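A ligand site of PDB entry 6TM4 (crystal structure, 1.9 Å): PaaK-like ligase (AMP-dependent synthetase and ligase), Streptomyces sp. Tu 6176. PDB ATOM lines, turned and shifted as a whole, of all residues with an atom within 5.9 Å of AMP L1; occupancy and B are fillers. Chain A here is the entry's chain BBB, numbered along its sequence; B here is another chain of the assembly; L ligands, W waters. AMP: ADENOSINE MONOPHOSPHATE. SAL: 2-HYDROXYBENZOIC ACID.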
ATOM      1  N   LYS A  63     -15.149  -2.610  -2.031  1.00  0.00           N
ATOM      2  CA  LYS A  63     -15.020  -2.610  -3.510  1.00  0.00           C
ATOM      3  C   LYS A  63     -14.931  -1.173  -4.004  1.00  0.00           C
ATOM      4  O   LYS A  63     -14.112  -0.927  -4.896  1.00  0.00           O
ATOM      5  CB  LYS A  63     -16.273  -3.181  -4.163  1.00  0.00           C
ATOM      6  CG  LYS A  63     -16.234  -4.663  -4.515  1.00  0.00           C
ATOM      7  CD  LYS A  63     -17.586  -5.109  -5.064  1.00  0.00           C
ATOM      8  CE  LYS A  63     -17.906  -6.575  -4.879  1.00  0.00           C
ATOM      9  NZ  LYS A  63     -17.186  -7.409  -5.859  1.00  0.00           N
ATOM     10  N   SER A  88     -11.080  -6.358 -13.136  1.00  0.00           N
ATOM     11  CA  SER A  88     -12.126  -7.310 -12.708  1.00  0.00           C
ATOM     12  C   SER A  88     -13.177  -7.409 -13.826  1.00  0.00           C
ATOM     13  O   SER A  88     -13.249  -6.483 -14.672  1.00  0.00           O
ATOM     14  CB  SER A  88     -12.702  -6.906 -11.356  1.00  0.00           C
ATOM     15  OG  SER A  88     -11.732  -7.173 -10.312  1.00  0.00           O
ATOM     16  N   SER A  89     -13.966  -8.480 -13.811  1.00  0.00           N
ATOM     17  CA  SER A  89     -15.195  -8.614 -14.636  1.00  0.00           C
ATOM     18  C   SER A  89     -16.263  -7.662 -14.070  1.00  0.00           C
ATOM     19  O   SER A  89     -15.937  -6.917 -13.128  1.00  0.00           O
ATOM     20  CB  SER A  89     -15.697 -10.065 -14.719  1.00  0.00           C
ATOM     21  OG  SER A  89     -16.213 -10.519 -13.482  1.00  0.00           O
ATOM     22  N   GLY A  90     -17.455  -7.656 -14.664  1.00  0.00           N
ATOM     23  CA  GLY A  90     -18.531  -6.713 -14.314  1.00  0.00           C
ATOM     24  C   GLY A  90     -18.425  -5.446 -15.144  1.00  0.00           C
ATOM     25  O   GLY A  90     -17.880  -5.526 -16.305  1.00  0.00           O
ATOM     26  N   VAL A 134      -8.709  -9.831 -17.320  1.00  0.00           N
ATOM     27  CA  VAL A 134      -9.033 -10.638 -16.106  1.00  0.00           C
ATOM     28  C   VAL A 134      -7.912 -11.643 -15.835  1.00  0.00           C
ATOM     29  O   VAL A 134      -7.117 -11.980 -16.765  1.00  0.00           O
ATOM     30  CB  VAL A 134     -10.413 -11.319 -16.226  1.00  0.00           C
ATOM     31  CG1 VAL A 134     -11.528 -10.285 -16.332  1.00  0.00           C
ATOM     32  CG2 VAL A 134     -10.473 -12.299 -17.380  1.00  0.00           C
ATOM     33  N   THR A 211     -13.762 -25.639 -12.208  1.00  0.00           N
ATOM     34  CA  THR A 211     -14.782 -24.625 -12.519  1.00  0.00           C
ATOM     35  C   THR A 211     -14.890 -23.627 -11.366  1.00  0.00           C
ATOM     36  O   THR A 211     -14.367 -23.924 -10.281  1.00  0.00           O
ATOM     37  CB  THR A 211     -16.116 -25.280 -12.861  1.00  0.00           C
ATOM     38  OG1 THR A 211     -16.919 -24.318 -13.541  1.00  0.00           O
ATOM     39  CG2 THR A 211     -16.848 -25.792 -11.652  1.00  0.00           C
ATOM     40  N   ALA A 212     -15.463 -22.455 -11.646  1.00  0.00           N
ATOM     41  CA  ALA A 212     -15.675 -21.329 -10.718  1.00  0.00           C
ATOM     42  C   ALA A 212     -16.552 -20.306 -11.397  1.00  0.00           C
ATOM     43  O   ALA A 212     -16.892 -20.548 -12.577  1.00  0.00           O
ATOM     44  CB  ALA A 212     -14.370 -20.690 -10.359  1.00  0.00           C
ATOM     45  N   ALA A 213     -16.797 -19.175 -10.709  1.00  0.00           N
ATOM     46  CA  ALA A 213     -17.201 -17.875 -11.287  1.00  0.00           C
ATOM     47  C   ALA A 213     -18.727 -17.723 -11.276  1.00  0.00           C
ATOM     48  O   ALA A 213     -19.168 -16.621 -11.573  1.00  0.00           O
ATOM     49  CB  ALA A 213     -16.651 -17.706 -12.694  1.00  0.00           C
ATOM     50  N   GLU A 214     -19.467 -18.799 -11.030  1.00  0.00           N
ATOM     51  CA  GLU A 214     -20.952 -18.811 -10.916  1.00  0.00           C
ATOM     52  C   GLU A 214     -21.327 -19.519  -9.633  1.00  0.00           C
ATOM     53  O   GLU A 214     -20.704 -20.514  -9.290  1.00  0.00           O
ATOM     54  CB  GLU A 214     -21.634 -19.650 -12.020  1.00  0.00           C
ATOM     55  CG  GLU A 214     -21.708 -18.992 -13.377  1.00  0.00           C
ATOM     56  CD  GLU A 214     -22.359 -19.889 -14.427  1.00  0.00           C
ATOM     57  OE1 GLU A 214     -21.732 -20.086 -15.497  1.00  0.00           O
ATOM     58  OE2 GLU A 214     -23.488 -20.364 -14.184  1.00  0.00           O
ATOM     59  N   PRO A 215     -22.368 -19.047  -8.929  1.00  0.00           N
ATOM     60  CA  PRO A 215     -22.956 -19.820  -7.844  1.00  0.00           C
ATOM     61  C   PRO A 215     -23.374 -21.196  -8.409  1.00  0.00           C
ATOM     62  O   PRO A 215     -24.013 -21.222  -9.460  1.00  0.00           O
ATOM     63  CB  PRO A 215     -24.163 -18.999  -7.372  1.00  0.00           C
ATOM     64  CG  PRO A 215     -23.969 -17.618  -7.989  1.00  0.00           C
ATOM     65  CD  PRO A 215     -23.059 -17.773  -9.187  1.00  0.00           C
ATOM     66  N   LEU A 216     -22.920 -22.280  -7.804  1.00  0.00           N
ATOM     67  CA  LEU A 216     -23.094 -23.638  -8.395  1.00  0.00           C
ATOM     68  C   LEU A 216     -23.680 -24.590  -7.342  1.00  0.00           C
ATOM     69  O   LEU A 216     -22.957 -24.917  -6.394  1.00  0.00           O
ATOM     70  CB  LEU A 216     -21.744 -24.144  -8.926  1.00  0.00           C
ATOM     71  CG  LEU A 216     -21.792 -25.507  -9.616  1.00  0.00           C
ATOM     72  CD1 LEU A 216     -22.697 -25.449 -10.834  1.00  0.00           C
ATOM     73  CD2 LEU A 216     -20.393 -25.956  -9.985  1.00  0.00           C
ATOM     74  N   GLU A 235     -14.805 -27.446  -8.053  1.00  0.00           N
ATOM     75  CA  GLU A 235     -15.128 -26.016  -7.885  1.00  0.00           C
ATOM     76  C   GLU A 235     -14.017 -25.308  -7.119  1.00  0.00           C
ATOM     77  O   GLU A 235     -13.503 -25.887  -6.147  1.00  0.00           O
ATOM     78  CB  GLU A 235     -16.438 -25.887  -7.135  1.00  0.00           C
ATOM     79  CG  GLU A 235     -17.174 -24.609  -7.460  1.00  0.00           C
ATOM     80  CD  GLU A 235     -18.378 -24.376  -6.568  1.00  0.00           C
ATOM     81  OE1 GLU A 235     -18.773 -25.336  -5.856  1.00  0.00           O
ATOM     82  OE2 GLU A 235     -18.870 -23.243  -6.554  1.00  0.00           O
ATOM     83  N   GLU A 236     -13.718 -24.075  -7.501  1.00  0.00           N
ATOM     84  CA  GLU A 236     -13.053 -23.119  -6.588  1.00  0.00           C
ATOM     85  C   GLU A 236     -13.810 -21.794  -6.537  1.00  0.00           C
ATOM     86  O   GLU A 236     -14.753 -21.583  -7.332  1.00  0.00           O
ATOM     87  CB  GLU A 236     -11.584 -22.911  -6.948  1.00  0.00           C
ATOM     88  CG  GLU A 236     -11.364 -22.280  -8.297  1.00  0.00           C
ATOM     89  CD  GLU A 236      -9.894 -21.908  -8.458  1.00  0.00           C
ATOM     90  OE1 GLU A 236      -9.042 -22.799  -8.426  1.00  0.00           O
ATOM     91  OE2 GLU A 236      -9.580 -20.692  -8.438  1.00  0.00           O
ATOM     92  N   TYR A 237     -13.436 -20.973  -5.566  1.00  0.00           N
ATOM     93  CA  TYR A 237     -13.991 -19.629  -5.319  1.00  0.00           C
ATOM     94  C   TYR A 237     -12.836 -18.637  -5.223  1.00  0.00           C
ATOM     95  O   TYR A 237     -11.846 -18.916  -4.484  1.00  0.00           O
ATOM     96  CB  TYR A 237     -14.807 -19.657  -4.043  1.00  0.00           C
ATOM     97  CG  TYR A 237     -15.251 -18.334  -3.502  1.00  0.00           C
ATOM     98  CD1 TYR A 237     -15.837 -17.361  -4.304  1.00  0.00           C
ATOM     99  CD2 TYR A 237     -15.173 -18.086  -2.146  1.00  0.00           C
ATOM    100  CE1 TYR A 237     -16.325 -16.183  -3.768  1.00  0.00           C
ATOM    101  CE2 TYR A 237     -15.646 -16.910  -1.593  1.00  0.00           C
ATOM    102  CZ  TYR A 237     -16.232 -15.954  -2.410  1.00  0.00           C
ATOM    103  OH  TYR A 237     -16.661 -14.802  -1.822  1.00  0.00           O
ATOM    104  N   GLY A 238     -12.925 -17.570  -5.993  1.00  0.00           N
ATOM    105  CA  GLY A 238     -11.994 -16.433  -5.914  1.00  0.00           C
ATOM    106  C   GLY A 238     -12.536 -15.187  -6.599  1.00  0.00           C
ATOM    107  O   GLY A 238     -13.739 -15.113  -6.821  1.00  0.00           O
ATOM    108  N   SER A 239     -11.638 -14.266  -6.914  1.00  0.00           N
ATOM    109  CA  SER A 239     -11.897 -12.965  -7.564  1.00  0.00           C
ATOM    110  C   SER A 239     -10.580 -12.465  -8.159  1.00  0.00           C
ATOM    111  O   SER A 239      -9.527 -12.918  -7.689  1.00  0.00           O
ATOM    112  CB  SER A 239     -12.441 -11.982  -6.545  1.00  0.00           C
ATOM    113  OG  SER A 239     -11.399 -11.484  -5.712  1.00  0.00           O
ATOM    114  N   THR A 240     -10.602 -11.546  -9.132  1.00  0.00           N
ATOM    115  CA  THR A 240      -9.367 -10.965  -9.740  1.00  0.00           C
ATOM    116  C   THR A 240      -8.467 -10.338  -8.663  1.00  0.00           C
ATOM    117  O   THR A 240      -7.191 -10.463  -8.763  1.00  0.00           O
ATOM    118  CB  THR A 240      -9.709  -9.890 -10.754  1.00  0.00           C
ATOM    119  OG1 THR A 240     -10.849 -10.428 -11.435  1.00  0.00           O
ATOM    120  CG2 THR A 240      -8.565  -9.575 -11.693  1.00  0.00           C
ATOM    121  N   GLU A 241      -9.109  -9.761  -7.650  1.00  0.00           N
ATOM    122  CA  GLU A 241      -8.451  -8.939  -6.622  1.00  0.00           C
ATOM    123  C   GLU A 241      -7.778  -9.822  -5.574  1.00  0.00           C
ATOM    124  O   GLU A 241      -6.917  -9.258  -4.842  1.00  0.00           O
ATOM    125  CB  GLU A 241      -9.456  -8.044  -5.893  1.00  0.00           C
ATOM    126  CG  GLU A 241     -10.406  -7.303  -6.802  1.00  0.00           C
ATOM    127  CD  GLU A 241     -11.725  -7.980  -7.077  1.00  0.00           C
ATOM    128  OE1 GLU A 241     -11.877  -8.494  -8.183  1.00  0.00           O
ATOM    129  OE2 GLU A 241     -12.637  -7.945  -6.205  1.00  0.00           O
ATOM    130  N   MET A 254     -16.108 -26.710  -0.591  1.00  0.00           N
ATOM    131  CA  MET A 254     -15.006 -25.743  -0.768  1.00  0.00           C
ATOM    132  C   MET A 254     -14.465 -25.392   0.615  1.00  0.00           C
ATOM    133  O   MET A 254     -15.256 -25.046   1.514  1.00  0.00           O
ATOM    134  CB  MET A 254     -15.442 -24.479  -1.525  1.00  0.00           C
ATOM    135  CG  MET A 254     -15.814 -24.790  -2.955  1.00  0.00           C
ATOM    136  SD  MET A 254     -15.913 -23.324  -4.009  1.00  0.00           S
ATOM    137  CE  MET A 254     -17.428 -22.608  -3.377  1.00  0.00           C
ATOM    138  N   LEU A 298     -15.369  -8.629  -0.268  1.00  0.00           N
ATOM    139  CA  LEU A 298     -15.826  -9.096  -1.603  1.00  0.00           C
ATOM    140  C   LEU A 298     -17.325  -8.850  -1.829  1.00  0.00           C
ATOM    141  O   LEU A 298     -17.735  -8.927  -2.998  1.00  0.00           O
ATOM    142  CB  LEU A 298     -15.563 -10.598  -1.759  1.00  0.00           C
ATOM    143  CG  LEU A 298     -14.212 -10.952  -2.336  1.00  0.00           C
ATOM    144  CD1 LEU A 298     -13.137 -10.547  -1.353  1.00  0.00           C
ATOM    145  CD2 LEU A 298     -14.128 -12.438  -2.620  1.00  0.00           C
ATOM    146  N   ASP A 300     -19.703 -10.835  -1.456  1.00  0.00           N
ATOM    147  CA  ASP A 300     -20.405 -12.094  -1.769  1.00  0.00           C
ATOM    148  C   ASP A 300     -21.087 -12.564  -0.478  1.00  0.00           C
ATOM    149  O   ASP A 300     -20.480 -12.411   0.617  1.00  0.00           O
ATOM    150  CB  ASP A 300     -19.460 -13.182  -2.263  1.00  0.00           C
ATOM    151  CG  ASP A 300     -18.844 -12.874  -3.595  1.00  0.00           C
ATOM    152  OD1 ASP A 300     -19.572 -12.301  -4.453  1.00  0.00           O
ATOM    153  OD2 ASP A 300     -17.670 -13.263  -3.796  1.00  0.00           O
ATOM    154  N   VAL A 320     -21.053 -20.347  -1.233  1.00  0.00           N
ATOM    155  CA  VAL A 320     -21.213 -19.010  -1.887  1.00  0.00           C
ATOM    156  C   VAL A 320     -22.617 -18.963  -2.516  1.00  0.00           C
ATOM    157  O   VAL A 320     -22.848 -19.694  -3.510  1.00  0.00           O
ATOM    158  CB  VAL A 320     -20.121 -18.782  -2.947  1.00  0.00           C
ATOM    159  CG1 VAL A 320     -20.259 -17.391  -3.560  1.00  0.00           C
ATOM    160  CG2 VAL A 320     -18.732 -19.012  -2.401  1.00  0.00           C
ATOM    161  N   GLY A 322     -24.195 -15.877  -3.632  1.00  0.00           N
ATOM    162  CA  GLY A 322     -24.226 -14.826  -4.670  1.00  0.00           C
ATOM    163  C   GLY A 322     -24.984 -13.597  -4.195  1.00  0.00           C
ATOM    164  O   GLY A 322     -24.288 -12.637  -3.762  1.00  0.00           O
ATOM    165  N   LYS B 418     -21.019 -12.664 -16.547  1.00  0.00           N
ATOM    166  CA  LYS B 418     -21.073 -14.116 -16.341  1.00  0.00           C
ATOM    167  C   LYS B 418     -22.521 -14.544 -16.620  1.00  0.00           C
ATOM    168  O   LYS B 418     -23.406 -13.700 -16.594  1.00  0.00           O
ATOM    169  CB  LYS B 418     -20.572 -14.440 -14.931  1.00  0.00           C
ATOM    170  CG  LYS B 418     -19.132 -13.994 -14.667  1.00  0.00           C
ATOM    171  CD  LYS B 418     -18.536 -14.622 -13.422  1.00  0.00           C
ATOM    172  CE  LYS B 418     -17.636 -13.725 -12.589  1.00  0.00           C
ATOM    173  NZ  LYS B 418     -18.438 -12.901 -11.647  1.00  0.00           N
HETATM  174  P   AMP L   1     -14.108 -11.122 -10.794  1.00  0.00           P
HETATM  175  O1P AMP L   1     -12.865 -10.748  -9.973  1.00  0.00           O
HETATM  176  O2P AMP L   1     -13.790 -12.192 -11.829  1.00  0.00           O
HETATM  177  O3P AMP L   1     -14.839  -9.932 -11.428  1.00  0.00           O
HETATM  178  O5' AMP L   1     -15.256 -11.618  -9.767  1.00  0.00           O
HETATM  179  C5' AMP L   1     -15.133 -12.792  -8.928  1.00  0.00           C
HETATM  180  C4' AMP L   1     -16.511 -13.084  -8.378  1.00  0.00           C
HETATM  181  O4' AMP L   1     -17.131 -14.220  -9.062  1.00  0.00           O
HETATM  182  C3' AMP L   1     -16.613 -13.450  -6.893  1.00  0.00           C
HETATM  183  O3' AMP L   1     -16.480 -12.315  -6.046  1.00  0.00           O
HETATM  184  C2' AMP L   1     -18.011 -14.068  -6.883  1.00  0.00           C
HETATM  185  O2' AMP L   1     -19.036 -13.098  -6.931  1.00  0.00           O
HETATM  186  C1' AMP L   1     -17.982 -14.899  -8.177  1.00  0.00           C
HETATM  187  N9  AMP L   1     -17.491 -16.268  -8.001  1.00  0.00           N
HETATM  188  C8  AMP L   1     -16.235 -16.773  -8.276  1.00  0.00           C
HETATM  189  N7  AMP L   1     -16.116 -18.063  -8.034  1.00  0.00           N
HETATM  190  C5  AMP L   1     -17.377 -18.440  -7.573  1.00  0.00           C
HETATM  191  C6  AMP L   1     -17.909 -19.686  -7.144  1.00  0.00           C
HETATM  192  N6  AMP L   1     -17.246 -20.831  -7.125  1.00  0.00           N
HETATM  193  N1  AMP L   1     -19.209 -19.706  -6.727  1.00  0.00           N
HETATM  194  C2  AMP L   1     -19.916 -18.555  -6.755  1.00  0.00           C
HETATM  195  N3  AMP L   1     -19.530 -17.331  -7.144  1.00  0.00           N
HETATM  196  C4  AMP L   1     -18.233 -17.337  -7.544  1.00  0.00           C
HETATM  197  C1' SAL L   2     -12.802 -15.000 -10.740  1.00  0.00           C
HETATM  198  O1' SAL L   2     -14.068 -15.207 -10.557  1.00  0.00           O
HETATM  199  O2' SAL L   2     -12.230 -14.077 -11.397  1.00  0.00           O
HETATM  200  C1  SAL L   2     -11.823 -15.937 -10.157  1.00  0.00           C
HETATM  201  C2  SAL L   2     -12.263 -17.241  -9.637  1.00  0.00           C
HETATM  202  C3  SAL L   2     -11.376 -18.158  -9.108  1.00  0.00           C
HETATM  203  C4  SAL L   2     -10.052 -17.760  -9.078  1.00  0.00           C
HETATM  204  C5  SAL L   2      -9.656 -16.508  -9.561  1.00  0.00           C
HETATM  205  C6  SAL L   2     -10.508 -15.579 -10.136  1.00  0.00           C
HETATM  206  O2  SAL L   2     -13.542 -17.547  -9.724  1.00  0.00           O
HETATM  207  C1' SAL L   3     -15.142 -17.051 -17.082  1.00  0.00           C
HETATM  208  O1' SAL L   3     -15.174 -18.018 -17.762  1.00  0.00           O
HETATM  209  O2' SAL L   3     -15.621 -15.966 -17.366  1.00  0.00           O
HETATM  210  C1  SAL L   3     -14.502 -17.200 -15.787  1.00  0.00           C
HETATM  211  C2  SAL L   3     -14.258 -15.998 -14.980  1.00  0.00           C
HETATM  212  C3  SAL L   3     -13.684 -16.158 -13.730  1.00  0.00           C
HETATM  213  C4  SAL L   3     -13.328 -17.440 -13.263  1.00  0.00           C
HETATM  214  C5  SAL L   3     -13.575 -18.594 -14.043  1.00  0.00           C
HETATM  215  C6  SAL L   3     -14.164 -18.469 -15.315  1.00  0.00           C
HETATM  216  O2  SAL L   3     -14.599 -14.776 -15.467  1.00  0.00           O
HETATM  217  O   HOH W   1     -18.644 -22.307  -9.527  1.00  0.00           O
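The side-chain hydroxyl of Thr 240 sits at hydrogen-bond distance from an oxygen (O1P) of AMP L1 (2.5 Å).
The backbone NH (N) of Ser 89 is in hydrogen-bond range of an oxygen (O3P) of AMP L1, at 2.9 Å.
An oxygen (O4') of AMP L1 is in hydrogen-bond range of the side-chain amino group (NZ) of Lys 418 of chain B (3.2 Å).
N of Thr 240 is in hydrogen-bond range of O1P of AMP L1.
The side-chain carboxylate (OD1) of Asp 300 lies within hydrogen-bond range of an oxygen (O2') of AMP L1, 2.7 Å away.
The backbone carbonyl oxygen (O) of Glu 236 lies within hydrogen-bond range of a nitrogen (N6) of AMP L1, 2.6 Å away.
N of Ala 213 sits at hydrogen-bond distance from N7 of AMP L1, at 3.0 Å.
OE2 of Glu 235 lies within hydrogen-bond range of N6 of AMP L1 (3.0 Å).
The side-chain carboxylate (OE1) of Glu 241 sits close to an oxygen (O1P) of AMP L1.
The side-chain hydroxyl (OG) of Ser 89 is in hydrogen-bond range of an oxygen (O3P) of AMP L1, 2.5 Å away.
A nitrogen (N7) of AMP L1 sits at hydrogen-bond distance from an oxygen (O2) of SAL L2 (3.1 Å).
Water W1 lies within hydrogen-bond range of the backbone carbonyl oxygen of Glu 214 (2.7 Å), the side-chain carboxylate of Glu 235 (3.1 Å) and a nitrogen (N6) of AMP L1 (3.1 Å).
O of Glu 214 lies close to N1 of AMP L1, at 3.1 Å.
Ser 88 touches AMP L1 (CB to O3P, 3.7 Å).
Ala 212 touches AMP L1.
N of Pro 215 touches C2 of AMP L1 (3.3 Å).
Tyr 237 touches AMP L1.
Gly 238 touches AMP L1.
Ser 239 touches AMP L1.
CG1 of Val 320 touches C2 of AMP L1 (3.4 Å).
The nearest printed residue that does not touch AMP L1 is Met 254 (4.2 Å).
The side-chain carboxylate (OD2) of Asp 300 lies within hydrogen-bond range of the side-chain hydroxyl (OH) of Tyr 237 (2.7 Å).
N of Glu 236 sits at hydrogen-bond distance from O of Thr 211.
The side-chain hydroxyl (OG) of Ser 239 lies close to the backbone NH (N) of Glu 241, at 3.5 Å.
The backbone NH (N) of Tyr 237 is in hydrogen-bond range of the side-chain sulfur (SD) of Met 254, 3.8 Å away.
The side-chain carboxylate of Glu 241 is in hydrogen-bond range of the side-chain hydroxyl of Ser 88 (2.5 Å).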
